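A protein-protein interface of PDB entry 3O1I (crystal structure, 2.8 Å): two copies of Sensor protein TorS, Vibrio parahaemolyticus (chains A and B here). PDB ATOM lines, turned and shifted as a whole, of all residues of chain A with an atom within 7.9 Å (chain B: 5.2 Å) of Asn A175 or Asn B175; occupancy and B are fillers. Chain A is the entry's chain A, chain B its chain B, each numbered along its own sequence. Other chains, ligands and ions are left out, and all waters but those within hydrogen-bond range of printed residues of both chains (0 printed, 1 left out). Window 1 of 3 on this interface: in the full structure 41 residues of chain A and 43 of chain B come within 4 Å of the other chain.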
ATOM      1  N   SER A 108      -1.340  29.960 -23.242  1.00  0.00           N
ATOM      2  CA  SER A 108      -0.456  29.463 -22.201  1.00  0.00           C
ATOM      3  C   SER A 108       0.962  29.936 -22.411  1.00  0.00           C
ATOM      4  O   SER A 108       1.748  30.029 -21.465  1.00  0.00           O
ATOM      5  CB  SER A 108      -0.498  27.933 -22.151  1.00  0.00           C
ATOM      6  OG  SER A 108       0.171  27.381 -23.261  1.00  0.00           O
ATOM      7  N   GLU A 112       3.132  31.855 -19.707  1.00  0.00           N
ATOM      8  CA  GLU A 112       4.454  31.435 -19.282  1.00  0.00           C
ATOM      9  C   GLU A 112       5.421  32.622 -19.344  1.00  0.00           C
ATOM     10  O   GLU A 112       6.236  32.813 -18.429  1.00  0.00           O
ATOM     11  CB  GLU A 112       4.922  30.256 -20.145  1.00  0.00           C
ATOM     12  CG  GLU A 112       6.319  29.730 -19.853  1.00  0.00           C
ATOM     13  CD  GLU A 112       7.396  30.578 -20.507  1.00  0.00           C
ATOM     14  OE1 GLU A 112       7.238  30.893 -21.704  1.00  0.00           O
ATOM     15  OE2 GLU A 112       8.399  30.919 -19.842  1.00  0.00           O
ATOM     16  N   LEU A 168       6.984  27.343 -12.931  1.00  0.00           N
ATOM     17  CA  LEU A 168       7.146  25.938 -13.265  1.00  0.00           C
ATOM     18  C   LEU A 168       5.790  25.396 -13.671  1.00  0.00           C
ATOM     19  O   LEU A 168       5.680  24.648 -14.636  1.00  0.00           O
ATOM     20  CB  LEU A 168       7.701  25.144 -12.081  1.00  0.00           C
ATOM     21  CG  LEU A 168       9.207  25.296 -11.806  1.00  0.00           C
ATOM     22  CD1 LEU A 168       9.580  24.519 -10.549  1.00  0.00           C
ATOM     23  CD2 LEU A 168      10.028  24.804 -13.000  1.00  0.00           C
ATOM     24  N   LEU A 169       4.753  25.788 -12.945  1.00  0.00           N
ATOM     25  CA  LEU A 169       3.413  25.326 -13.265  1.00  0.00           C
ATOM     26  C   LEU A 169       2.952  25.801 -14.641  1.00  0.00           C
ATOM     27  O   LEU A 169       2.324  25.060 -15.400  1.00  0.00           O
ATOM     28  CB  LEU A 169       2.426  25.802 -12.208  1.00  0.00           C
ATOM     29  CG  LEU A 169       2.099  24.776 -11.135  1.00  0.00           C
ATOM     30  CD1 LEU A 169       3.324  24.493 -10.281  1.00  0.00           C
ATOM     31  CD2 LEU A 169       0.969  25.313 -10.288  1.00  0.00           C
ATOM     32  N   ALA A 170       3.260  27.042 -14.968  1.00  0.00           N
ATOM     33  CA  ALA A 170       2.843  27.561 -16.254  1.00  0.00           C
ATOM     34  C   ALA A 170       3.605  26.849 -17.373  1.00  0.00           C
ATOM     35  O   ALA A 170       3.055  26.571 -18.427  1.00  0.00           O
ATOM     36  CB  ALA A 170       3.076  29.077 -16.308  1.00  0.00           C
ATOM     37  N   PHE A 171       4.873  26.555 -17.129  1.00  0.00           N
ATOM     38  CA  PHE A 171       5.728  25.882 -18.103  1.00  0.00           C
ATOM     39  C   PHE A 171       5.208  24.447 -18.311  1.00  0.00           C
ATOM     40  O   PHE A 171       5.189  23.920 -19.429  1.00  0.00           O
ATOM     41  CB  PHE A 171       7.165  25.860 -17.561  1.00  0.00           C
ATOM     42  CG  PHE A 171       8.194  25.535 -18.587  1.00  0.00           C
ATOM     43  CD1 PHE A 171       8.629  26.507 -19.480  1.00  0.00           C
ATOM     44  CD2 PHE A 171       8.708  24.249 -18.690  1.00  0.00           C
ATOM     45  CE1 PHE A 171       9.562  26.205 -20.471  1.00  0.00           C
ATOM     46  CE2 PHE A 171       9.643  23.930 -19.671  1.00  0.00           C
ATOM     47  CZ  PHE A 171      10.073  24.912 -20.567  1.00  0.00           C
ATOM     48  N   LYS A 172       4.784  23.820 -17.220  1.00  0.00           N
ATOM     49  CA  LYS A 172       4.256  22.472 -17.285  1.00  0.00           C
ATOM     50  C   LYS A 172       3.028  22.510 -18.197  1.00  0.00           C
ATOM     51  O   LYS A 172       2.940  21.774 -19.185  1.00  0.00           O
ATOM     52  CB  LYS A 172       3.869  22.002 -15.883  1.00  0.00           C
ATOM     53  CG  LYS A 172       3.407  20.551 -15.813  1.00  0.00           C
ATOM     54  CD  LYS A 172       4.501  19.584 -16.286  1.00  0.00           C
ATOM     55  CE  LYS A 172       4.045  18.122 -16.190  1.00  0.00           C
ATOM     56  NZ  LYS A 172       5.185  17.155 -16.123  1.00  0.00           N
ATOM     57  N   MET A 173       2.094  23.392 -17.855  1.00  0.00           N
ATOM     58  CA  MET A 173       0.870  23.578 -18.612  1.00  0.00           C
ATOM     59  C   MET A 173       1.165  23.789 -20.100  1.00  0.00           C
ATOM     60  O   MET A 173       0.581  23.150 -20.976  1.00  0.00           O
ATOM     61  CB  MET A 173       0.112  24.778 -18.055  1.00  0.00           C
ATOM     62  CG  MET A 173      -1.071  25.209 -18.897  1.00  0.00           C
ATOM     63  SD  MET A 173      -2.173  26.298 -17.985  1.00  0.00           S
ATOM     64  CE  MET A 173      -2.024  25.585 -16.244  1.00  0.00           C
ATOM     65  N   LEU A 174       2.077  24.696 -20.383  1.00  0.00           N
ATOM     66  CA  LEU A 174       2.424  24.966 -21.748  1.00  0.00           C
ATOM     67  C   LEU A 174       2.913  23.691 -22.451  1.00  0.00           C
ATOM     68  O   LEU A 174       2.641  23.492 -23.638  1.00  0.00           O
ATOM     69  CB  LEU A 174       3.494  26.053 -21.796  1.00  0.00           C
ATOM     70  CG  LEU A 174       4.151  26.301 -23.160  1.00  0.00           C
ATOM     71  CD1 LEU A 174       3.089  26.541 -24.244  1.00  0.00           C
ATOM     72  CD2 LEU A 174       5.085  27.489 -23.032  1.00  0.00           C
ATOM     73  N   ASN A 175       3.621  22.824 -21.730  1.00  0.00           N
ATOM     74  CA  ASN A 175       4.130  21.604 -22.346  1.00  0.00           C
ATOM     75  C   ASN A 175       2.988  20.665 -22.655  1.00  0.00           C
ATOM     76  O   ASN A 175       2.959  20.025 -23.701  1.00  0.00           O
ATOM     77  CB  ASN A 175       5.144  20.899 -21.434  1.00  0.00           C
ATOM     78  CG  ASN A 175       6.554  21.445 -21.593  1.00  0.00           C
ATOM     79  OD1 ASN A 175       6.799  22.376 -22.371  1.00  0.00           O
ATOM     80  ND2 ASN A 175       7.493  20.864 -20.853  1.00  0.00           N
ATOM     81  N   GLN A 176       2.042  20.571 -21.736  1.00  0.00           N
ATOM     82  CA  GLN A 176       0.905  19.705 -21.958  1.00  0.00           C
ATOM     83  C   GLN A 176       0.168  20.114 -23.253  1.00  0.00           C
ATOM     84  O   GLN A 176      -0.144  19.273 -24.099  1.00  0.00           O
ATOM     85  CB  GLN A 176      -0.005  19.761 -20.738  1.00  0.00           C
ATOM     86  CG  GLN A 176       0.739  19.385 -19.482  1.00  0.00           C
ATOM     87  CD  GLN A 176      -0.135  19.369 -18.242  1.00  0.00           C
ATOM     88  OE1 GLN A 176      -0.849  20.333 -17.956  1.00  0.00           O
ATOM     89  NE2 GLN A 176      -0.070  18.275 -17.493  1.00  0.00           N
ATOM     90  N   ILE A 177      -0.090  21.402 -23.406  1.00  0.00           N
ATOM     91  CA  ILE A 177      -0.749  21.909 -24.596  1.00  0.00           C
ATOM     92  C   ILE A 177       0.110  21.620 -25.829  1.00  0.00           C
ATOM     93  O   ILE A 177      -0.396  21.204 -26.871  1.00  0.00           O
ATOM     94  CB  ILE A 177      -1.021  23.426 -24.435  1.00  0.00           C
ATOM     95  CG1 ILE A 177      -2.119  23.624 -23.395  1.00  0.00           C
ATOM     96  CG2 ILE A 177      -1.425  24.053 -25.746  1.00  0.00           C
ATOM     97  CD1 ILE A 177      -2.372  25.048 -23.095  1.00  0.00           C
ATOM     98  N   GLU A 178       1.415  21.807 -25.720  1.00  0.00           N
ATOM     99  CA  GLU A 178       2.265  21.522 -26.864  1.00  0.00           C
ATOM    100  C   GLU A 178       2.198  20.043 -27.283  1.00  0.00           C
ATOM    101  O   GLU A 178       2.353  19.708 -28.442  1.00  0.00           O
ATOM    102  CB  GLU A 178       3.716  21.927 -26.575  1.00  0.00           C
ATOM    103  CG  GLU A 178       3.921  23.426 -26.330  1.00  0.00           C
ATOM    104  CD  GLU A 178       5.364  23.796 -25.945  1.00  0.00           C
ATOM    105  OE1 GLU A 178       5.989  23.077 -25.128  1.00  0.00           O
ATOM    106  OE2 GLU A 178       5.872  24.826 -26.445  1.00  0.00           O
ATOM    107  N   GLU A 179       1.962  19.154 -26.335  1.00  0.00           N
ATOM    108  CA  GLU A 179       1.889  17.729 -26.632  1.00  0.00           C
ATOM    109  C   GLU A 179       0.517  17.321 -27.172  1.00  0.00           C
ATOM    110  O   GLU A 179       0.398  16.361 -27.932  1.00  0.00           O
ATOM    111  CB  GLU A 179       2.225  16.919 -25.365  1.00  0.00           C
ATOM    112  CG  GLU A 179       1.481  15.604 -25.242  1.00  0.00           C
ATOM    113  CD  GLU A 179       2.071  14.649 -24.208  1.00  0.00           C
ATOM    114  OE1 GLU A 179       2.531  15.099 -23.138  1.00  0.00           O
ATOM    115  OE2 GLU A 179       2.061  13.431 -24.462  1.00  0.00           O
ATOM    116  N   ALA A 180      -0.502  18.081 -26.788  1.00  0.00           N
ATOM    117  CA  ALA A 180      -1.884  17.824 -27.160  1.00  0.00           C
ATOM    118  C   ALA A 180      -2.231  17.766 -28.644  1.00  0.00           C
ATOM    119  O   ALA A 180      -3.081  16.974 -29.044  1.00  0.00           O
ATOM    120  CB  ALA A 180      -2.789  18.852 -26.468  1.00  0.00           C
ATOM    121  N   ARG A 181      -1.594  18.585 -29.470  1.00  0.00           N
ATOM    122  CA  ARG A 181      -1.971  18.569 -30.873  1.00  0.00           C
ATOM    123  C   ARG A 181      -1.692  17.275 -31.624  1.00  0.00           C
ATOM    124  O   ARG A 181      -2.222  17.082 -32.716  1.00  0.00           O
ATOM    125  CB  ARG A 181      -1.369  19.762 -31.644  1.00  0.00           C
ATOM    126  CG  ARG A 181       0.071  19.623 -32.083  1.00  0.00           C
ATOM    127  CD  ARG A 181       0.354  20.536 -33.282  1.00  0.00           C
ATOM    128  NE  ARG A 181      -0.411  20.107 -34.459  1.00  0.00           N
ATOM    129  CZ  ARG A 181       0.080  19.365 -35.456  1.00  0.00           C
ATOM    130  NH1 ARG A 181       1.351  18.965 -35.443  1.00  0.00           N
ATOM    131  NH2 ARG A 181      -0.709  18.984 -36.453  1.00  0.00           N
ATOM    132  N   ARG A 188      -3.040   8.401 -22.326  1.00  0.00           N
ATOM    133  CA  ARG A 188      -2.305   9.636 -22.166  1.00  0.00           C
ATOM    134  C   ARG A 188      -3.236  10.847 -22.252  1.00  0.00           C
ATOM    135  O   ARG A 188      -3.127  11.788 -21.467  1.00  0.00           O
ATOM    136  CB  ARG A 188      -1.226   9.716 -23.237  1.00  0.00           C
ATOM    137  CG  ARG A 188      -0.313  10.911 -23.106  1.00  0.00           C
ATOM    138  CD  ARG A 188       0.490  10.892 -21.834  1.00  0.00           C
ATOM    139  NE  ARG A 188       1.506  11.931 -21.916  1.00  0.00           N
ATOM    140  CZ  ARG A 188       2.124  12.481 -20.874  1.00  0.00           C
ATOM    141  NH1 ARG A 188       1.852  12.098 -19.639  1.00  0.00           N
ATOM    142  NH2 ARG A 188       2.988  13.461 -21.069  1.00  0.00           N
ATOM    143  N   ILE A 192      -3.223  13.639 -19.153  1.00  0.00           N
ATOM    144  CA  ILE A 192      -2.952  15.063 -19.310  1.00  0.00           C
ATOM    145  C   ILE A 192      -4.220  15.833 -18.956  1.00  0.00           C
ATOM    146  O   ILE A 192      -4.167  16.871 -18.295  1.00  0.00           O
ATOM    147  CB  ILE A 192      -2.579  15.457 -20.769  1.00  0.00           C
ATOM    148  CG1 ILE A 192      -1.387  14.650 -21.299  1.00  0.00           C
ATOM    149  CG2 ILE A 192      -2.227  16.939 -20.811  1.00  0.00           C
ATOM    150  CD1 ILE A 192      -0.041  15.090 -20.805  1.00  0.00           C
ATOM    151  N   PHE A 196      -3.987  18.564 -16.465  1.00  0.00           N
ATOM    152  CA  PHE A 196      -4.253  19.934 -16.890  1.00  0.00           C
ATOM    153  C   PHE A 196      -5.321  20.610 -16.048  1.00  0.00           C
ATOM    154  O   PHE A 196      -5.195  21.771 -15.707  1.00  0.00           O
ATOM    155  CB  PHE A 196      -4.676  19.977 -18.366  1.00  0.00           C
ATOM    156  CG  PHE A 196      -4.665  21.360 -18.953  1.00  0.00           C
ATOM    157  CD1 PHE A 196      -3.463  21.962 -19.330  1.00  0.00           C
ATOM    158  CD2 PHE A 196      -5.842  22.097 -19.050  1.00  0.00           C
ATOM    159  CE1 PHE A 196      -3.434  23.309 -19.793  1.00  0.00           C
ATOM    160  CE2 PHE A 196      -5.833  23.428 -19.502  1.00  0.00           C
ATOM    161  CZ  PHE A 196      -4.628  24.041 -19.876  1.00  0.00           C
ATOM    162  N   PHE B 171      13.756  20.200 -15.399  1.00  0.00           N
ATOM    163  CA  PHE B 171      12.323  19.957 -15.360  1.00  0.00           C
ATOM    164  C   PHE B 171      11.752  19.777 -16.764  1.00  0.00           C
ATOM    165  O   PHE B 171      10.924  18.893 -17.015  1.00  0.00           O
ATOM    166  CB  PHE B 171      11.650  21.139 -14.670  1.00  0.00           C
ATOM    167  CG  PHE B 171      10.166  21.037 -14.601  1.00  0.00           C
ATOM    168  CD1 PHE B 171       9.555  20.103 -13.766  1.00  0.00           C
ATOM    169  CD2 PHE B 171       9.370  21.912 -15.337  1.00  0.00           C
ATOM    170  CE1 PHE B 171       8.164  20.054 -13.659  1.00  0.00           C
ATOM    171  CE2 PHE B 171       7.979  21.871 -15.235  1.00  0.00           C
ATOM    172  CZ  PHE B 171       7.371  20.939 -14.394  1.00  0.00           C
ATOM    173  N   LYS B 172      12.202  20.647 -17.658  1.00  0.00           N
ATOM    174  CA  LYS B 172      11.810  20.656 -19.046  1.00  0.00           C
ATOM    175  C   LYS B 172      12.136  19.297 -19.680  1.00  0.00           C
ATOM    176  O   LYS B 172      11.413  18.822 -20.563  1.00  0.00           O
ATOM    177  CB  LYS B 172      12.576  21.782 -19.726  1.00  0.00           C
ATOM    178  CG  LYS B 172      12.708  21.676 -21.230  1.00  0.00           C
ATOM    179  CD  LYS B 172      13.426  22.916 -21.766  1.00  0.00           C
ATOM    180  CE  LYS B 172      13.522  22.899 -23.282  1.00  0.00           C
ATOM    181  NZ  LYS B 172      14.030  24.215 -23.759  1.00  0.00           N
ATOM    182  N   MET B 173      13.219  18.680 -19.202  1.00  0.00           N
ATOM    183  CA  MET B 173      13.697  17.396 -19.694  1.00  0.00           C
ATOM    184  C   MET B 173      12.840  16.241 -19.165  1.00  0.00           C
ATOM    185  O   MET B 173      12.539  15.278 -19.879  1.00  0.00           O
ATOM    186  CB  MET B 173      15.170  17.215 -19.295  1.00  0.00           C
ATOM    187  CG  MET B 173      15.796  15.894 -19.747  1.00  0.00           C
ATOM    188  SD  MET B 173      17.542  15.644 -19.288  1.00  0.00           S
ATOM    189  CE  MET B 173      18.328  17.251 -19.887  1.00  0.00           C
ATOM    190  N   LEU B 174      12.451  16.331 -17.904  1.00  0.00           N
ATOM    191  CA  LEU B 174      11.615  15.301 -17.336  1.00  0.00           C
ATOM    192  C   LEU B 174      10.312  15.282 -18.124  1.00  0.00           C
ATOM    193  O   LEU B 174       9.819  14.236 -18.502  1.00  0.00           O
ATOM    194  CB  LEU B 174      11.312  15.604 -15.875  1.00  0.00           C
ATOM    195  CG  LEU B 174      10.342  14.599 -15.251  1.00  0.00           C
ATOM    196  CD1 LEU B 174      10.910  13.149 -15.338  1.00  0.00           C
ATOM    197  CD2 LEU B 174      10.093  15.028 -13.821  1.00  0.00           C
ATOM    198  N   ASN B 175       9.764  16.463 -18.372  1.00  0.00           N
ATOM    199  CA  ASN B 175       8.512  16.581 -19.107  1.00  0.00           C
ATOM    200  C   ASN B 175       8.595  15.920 -20.489  1.00  0.00           C
ATOM    201  O   ASN B 175       7.654  15.228 -20.909  1.00  0.00           O
ATOM    202  CB  ASN B 175       8.112  18.060 -19.238  1.00  0.00           C
ATOM    203  CG  ASN B 175       7.665  18.672 -17.900  1.00  0.00           C
ATOM    204  OD1 ASN B 175       7.640  17.996 -16.857  1.00  0.00           O
ATOM    205  ND2 ASN B 175       7.312  19.957 -17.930  1.00  0.00           N
ATOM    206  N   GLN B 176       9.716  16.121 -21.184  1.00  0.00           N
ATOM    207  CA  GLN B 176       9.904  15.530 -22.503  1.00  0.00           C
ATOM    208  C   GLN B 176       9.901  14.018 -22.398  1.00  0.00           C
ATOM    209  O   GLN B 176       9.324  13.327 -23.230  1.00  0.00           O
ATOM    210  CB  GLN B 176      11.226  15.966 -23.103  1.00  0.00           C
ATOM    211  CG  GLN B 176      11.335  17.426 -23.318  1.00  0.00           C
ATOM    212  CD  GLN B 176      12.736  17.843 -23.677  1.00  0.00           C
ATOM    213  OE1 GLN B 176      13.704  17.449 -23.019  1.00  0.00           O
ATOM    214  NE2 GLN B 176      12.859  18.651 -24.722  1.00  0.00           N
ATOM    215  N   ILE B 177      10.557  13.501 -21.373  1.00  0.00           N
ATOM    216  CA  ILE B 177      10.623  12.065 -21.185  1.00  0.00           C
ATOM    217  C   ILE B 177       9.250  11.490 -20.863  1.00  0.00           C
ATOM    218  O   ILE B 177       8.884  10.422 -21.368  1.00  0.00           O
ATOM    219  CB  ILE B 177      11.643  11.716 -20.081  1.00  0.00           C
ATOM    220  CG1 ILE B 177      13.052  12.001 -20.593  1.00  0.00           C
ATOM    221  CG2 ILE B 177      11.523  10.263 -19.686  1.00  0.00           C
ATOM    222  CD1 ILE B 177      14.104  11.775 -19.564  1.00  0.00           C
ATOM    223  N   GLU B 178       8.490  12.199 -20.034  1.00  0.00           N
ATOM    224  CA  GLU B 178       7.154  11.760 -19.671  1.00  0.00           C
ATOM    225  C   GLU B 178       6.296  11.675 -20.934  1.00  0.00           C
ATOM    226  O   GLU B 178       5.338  10.906 -20.986  1.00  0.00           O
ATOM    227  CB  GLU B 178       6.510  12.743 -18.692  1.00  0.00           C
ATOM    228  CG  GLU B 178       7.227  12.905 -17.338  1.00  0.00           C
ATOM    229  CD  GLU B 178       6.561  13.944 -16.432  1.00  0.00           C
ATOM    230  OE1 GLU B 178       5.870  14.844 -16.961  1.00  0.00           O
ATOM    231  OE2 GLU B 178       6.740  13.877 -15.194  1.00  0.00           O
ATOM    232  N   GLU B 179       6.631  12.466 -21.953  1.00  0.00           N
ATOM    233  CA  GLU B 179       5.864  12.448 -23.199  1.00  0.00           C
ATOM    234  C   GLU B 179       6.360  11.354 -24.160  1.00  0.00           C
ATOM    235  O   GLU B 179       5.571  10.754 -24.900  1.00  0.00           O
ATOM    236  CB  GLU B 179       5.942  13.807 -23.916  1.00  0.00           C
ATOM    237  CG  GLU B 179       5.030  13.889 -25.153  1.00  0.00           C
ATOM    238  CD  GLU B 179       5.258  15.126 -26.012  1.00  0.00           C
ATOM    239  OE1 GLU B 179       5.875  16.094 -25.517  1.00  0.00           O
ATOM    240  OE2 GLU B 179       4.808  15.135 -27.182  1.00  0.00           O
ATOM    241  N   ARG B 188       6.502  15.152 -34.274  1.00  0.00           N
ATOM    242  CA  ARG B 188       6.662  15.439 -32.871  1.00  0.00           C
ATOM    243  C   ARG B 188       7.864  14.710 -32.298  1.00  0.00           C
ATOM    244  O   ARG B 188       8.607  15.273 -31.497  1.00  0.00           O
ATOM    245  CB  ARG B 188       5.385  15.058 -32.124  1.00  0.00           C
ATOM    246  CG  ARG B 188       5.454  15.267 -30.616  1.00  0.00           C
ATOM    247  CD  ARG B 188       5.663  16.724 -30.269  1.00  0.00           C
ATOM    248  NE  ARG B 188       5.429  16.976 -28.851  1.00  0.00           N
ATOM    249  CZ  ARG B 188       5.717  18.123 -28.250  1.00  0.00           C
ATOM    250  NH1 ARG B 188       6.257  19.113 -28.949  1.00  0.00           N
ATOM    251  NH2 ARG B 188       5.454  18.283 -26.959  1.00  0.00           N
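The side-chain amino group (NZ) of Lys A172 is in hydrogen-bond range of the side-chain amide oxygen (OD1) of Asn B175 (2.7 Å).
The side-chain carboxylate (OE1) of Glu B178 lies within salt-bridge range of the side-chain amino group (NZ) of Lys A172.
The side-chain amide nitrogen (ND2) of Asn A175 lies close to the side-chain amide nitrogen (ND2) of Asn B175 (3.1 Å).
O of Glu B178 sits at hydrogen-bond distance from NH2 of Arg A188, 3.5 Å away.
The side-chain amide oxygen (OD1) of Asn A175 lies close to the side-chain carboxylate (OE1) of Glu A178 (3.0 Å).
The side-chain carboxylate of Glu A179 lies within salt-bridge range of the guanidinium group of Arg A188, 2.7 Å away.
O of Phe B171 sits close to OD1 of Asn B175, at 3.4 Å.
The guanidinium group (NE) of Arg B188 lies within salt-bridge range of the side-chain carboxylate (OE2) of Glu B179, 2.6 Å away.
Leu A168 touches Phe B171 (O to CE2, 3.7 Å).
CE2 of Phe A171 touches CB of Lys B172, at 3.6 Å.
Lys A172 touches Phe B171 (CD to CZ, 3.7 Å).
Glu A178 touches Arg B188 (C to NH2, 3.7 Å).
Glu B179 touches Glu A179.
Arg B188 touches Glu A179.
Glu B179 touches Arg A188.
Of chain B, only Asn B175 (3.1 Å) comes within 4 Å of Asn A175.
Of chain A, only Lys A172 (2.7 Å) and Asn A175 (3.1 Å) come within 4 Å of Asn B175.
Of the printed residues of chain A, Glu B178 touches Lys A172 (2.6 Å) and Arg A188 (3.5 Å).
Printed residues of chain B within 4 Å of Glu A179: Glu B179 and Arg B188.
Printed residues of chain A within 4 Å of Phe B171: Leu A168 (3.7 Å) and Lys A172 (3.7 Å).
Printed residues of chain B within 4 Å of Leu A168: Phe B171.
Glu A112 touches none of the printed residues of chain B.
The nearest printed residue of chain B that does not touch Asn A175 is Lys B172 (4.4 Å).
The nearest residue of chain A that does not touch Asn B175 is Phe A171 (4.6 Å).
The nearest printed residue of chain B that does not touch Arg A188 is Asn B175 (5.0 Å).
Printed residues of chain B that touch a printed residue of chain A: Phe B171, Lys B172, Asn B175, Glu B178, Glu B179 and Arg B188.
Hydrophobic or aromatic side chains of chain B within 4 Å of the printed part of chain A: Phe B171.
Hydrophobic or aromatic side chains of chain A that line the printed part of chain B: Leu A168 and Phe A171.
Along chain A the printed residues that touch a printed residue of chain B span positions 168 to 188.
Among the printed residues, 11 pairs touch across the chains.
Among the printed residues, Asp or Glu carboxylates within 4 Å of a Lys or Arg side-chain nitrogen of the other chain: Lys A172 with Glu B178 (2.6 Å).
Lys A172 touches Glu B178, but with the chains exchanged Glu A178 does not touch Lys B172 (7.8 Å).
Asn A175 touches its own counterpart, Asn B175.
Glu A178 touches Arg B188, and with the chains exchanged Arg A188 touches Glu B178.
Glu A179 touches its own counterpart, Glu B179.
Of the 11 pairs that touch across the chains among the printed residues, 8 have their exchanged pair printed and touching as well.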
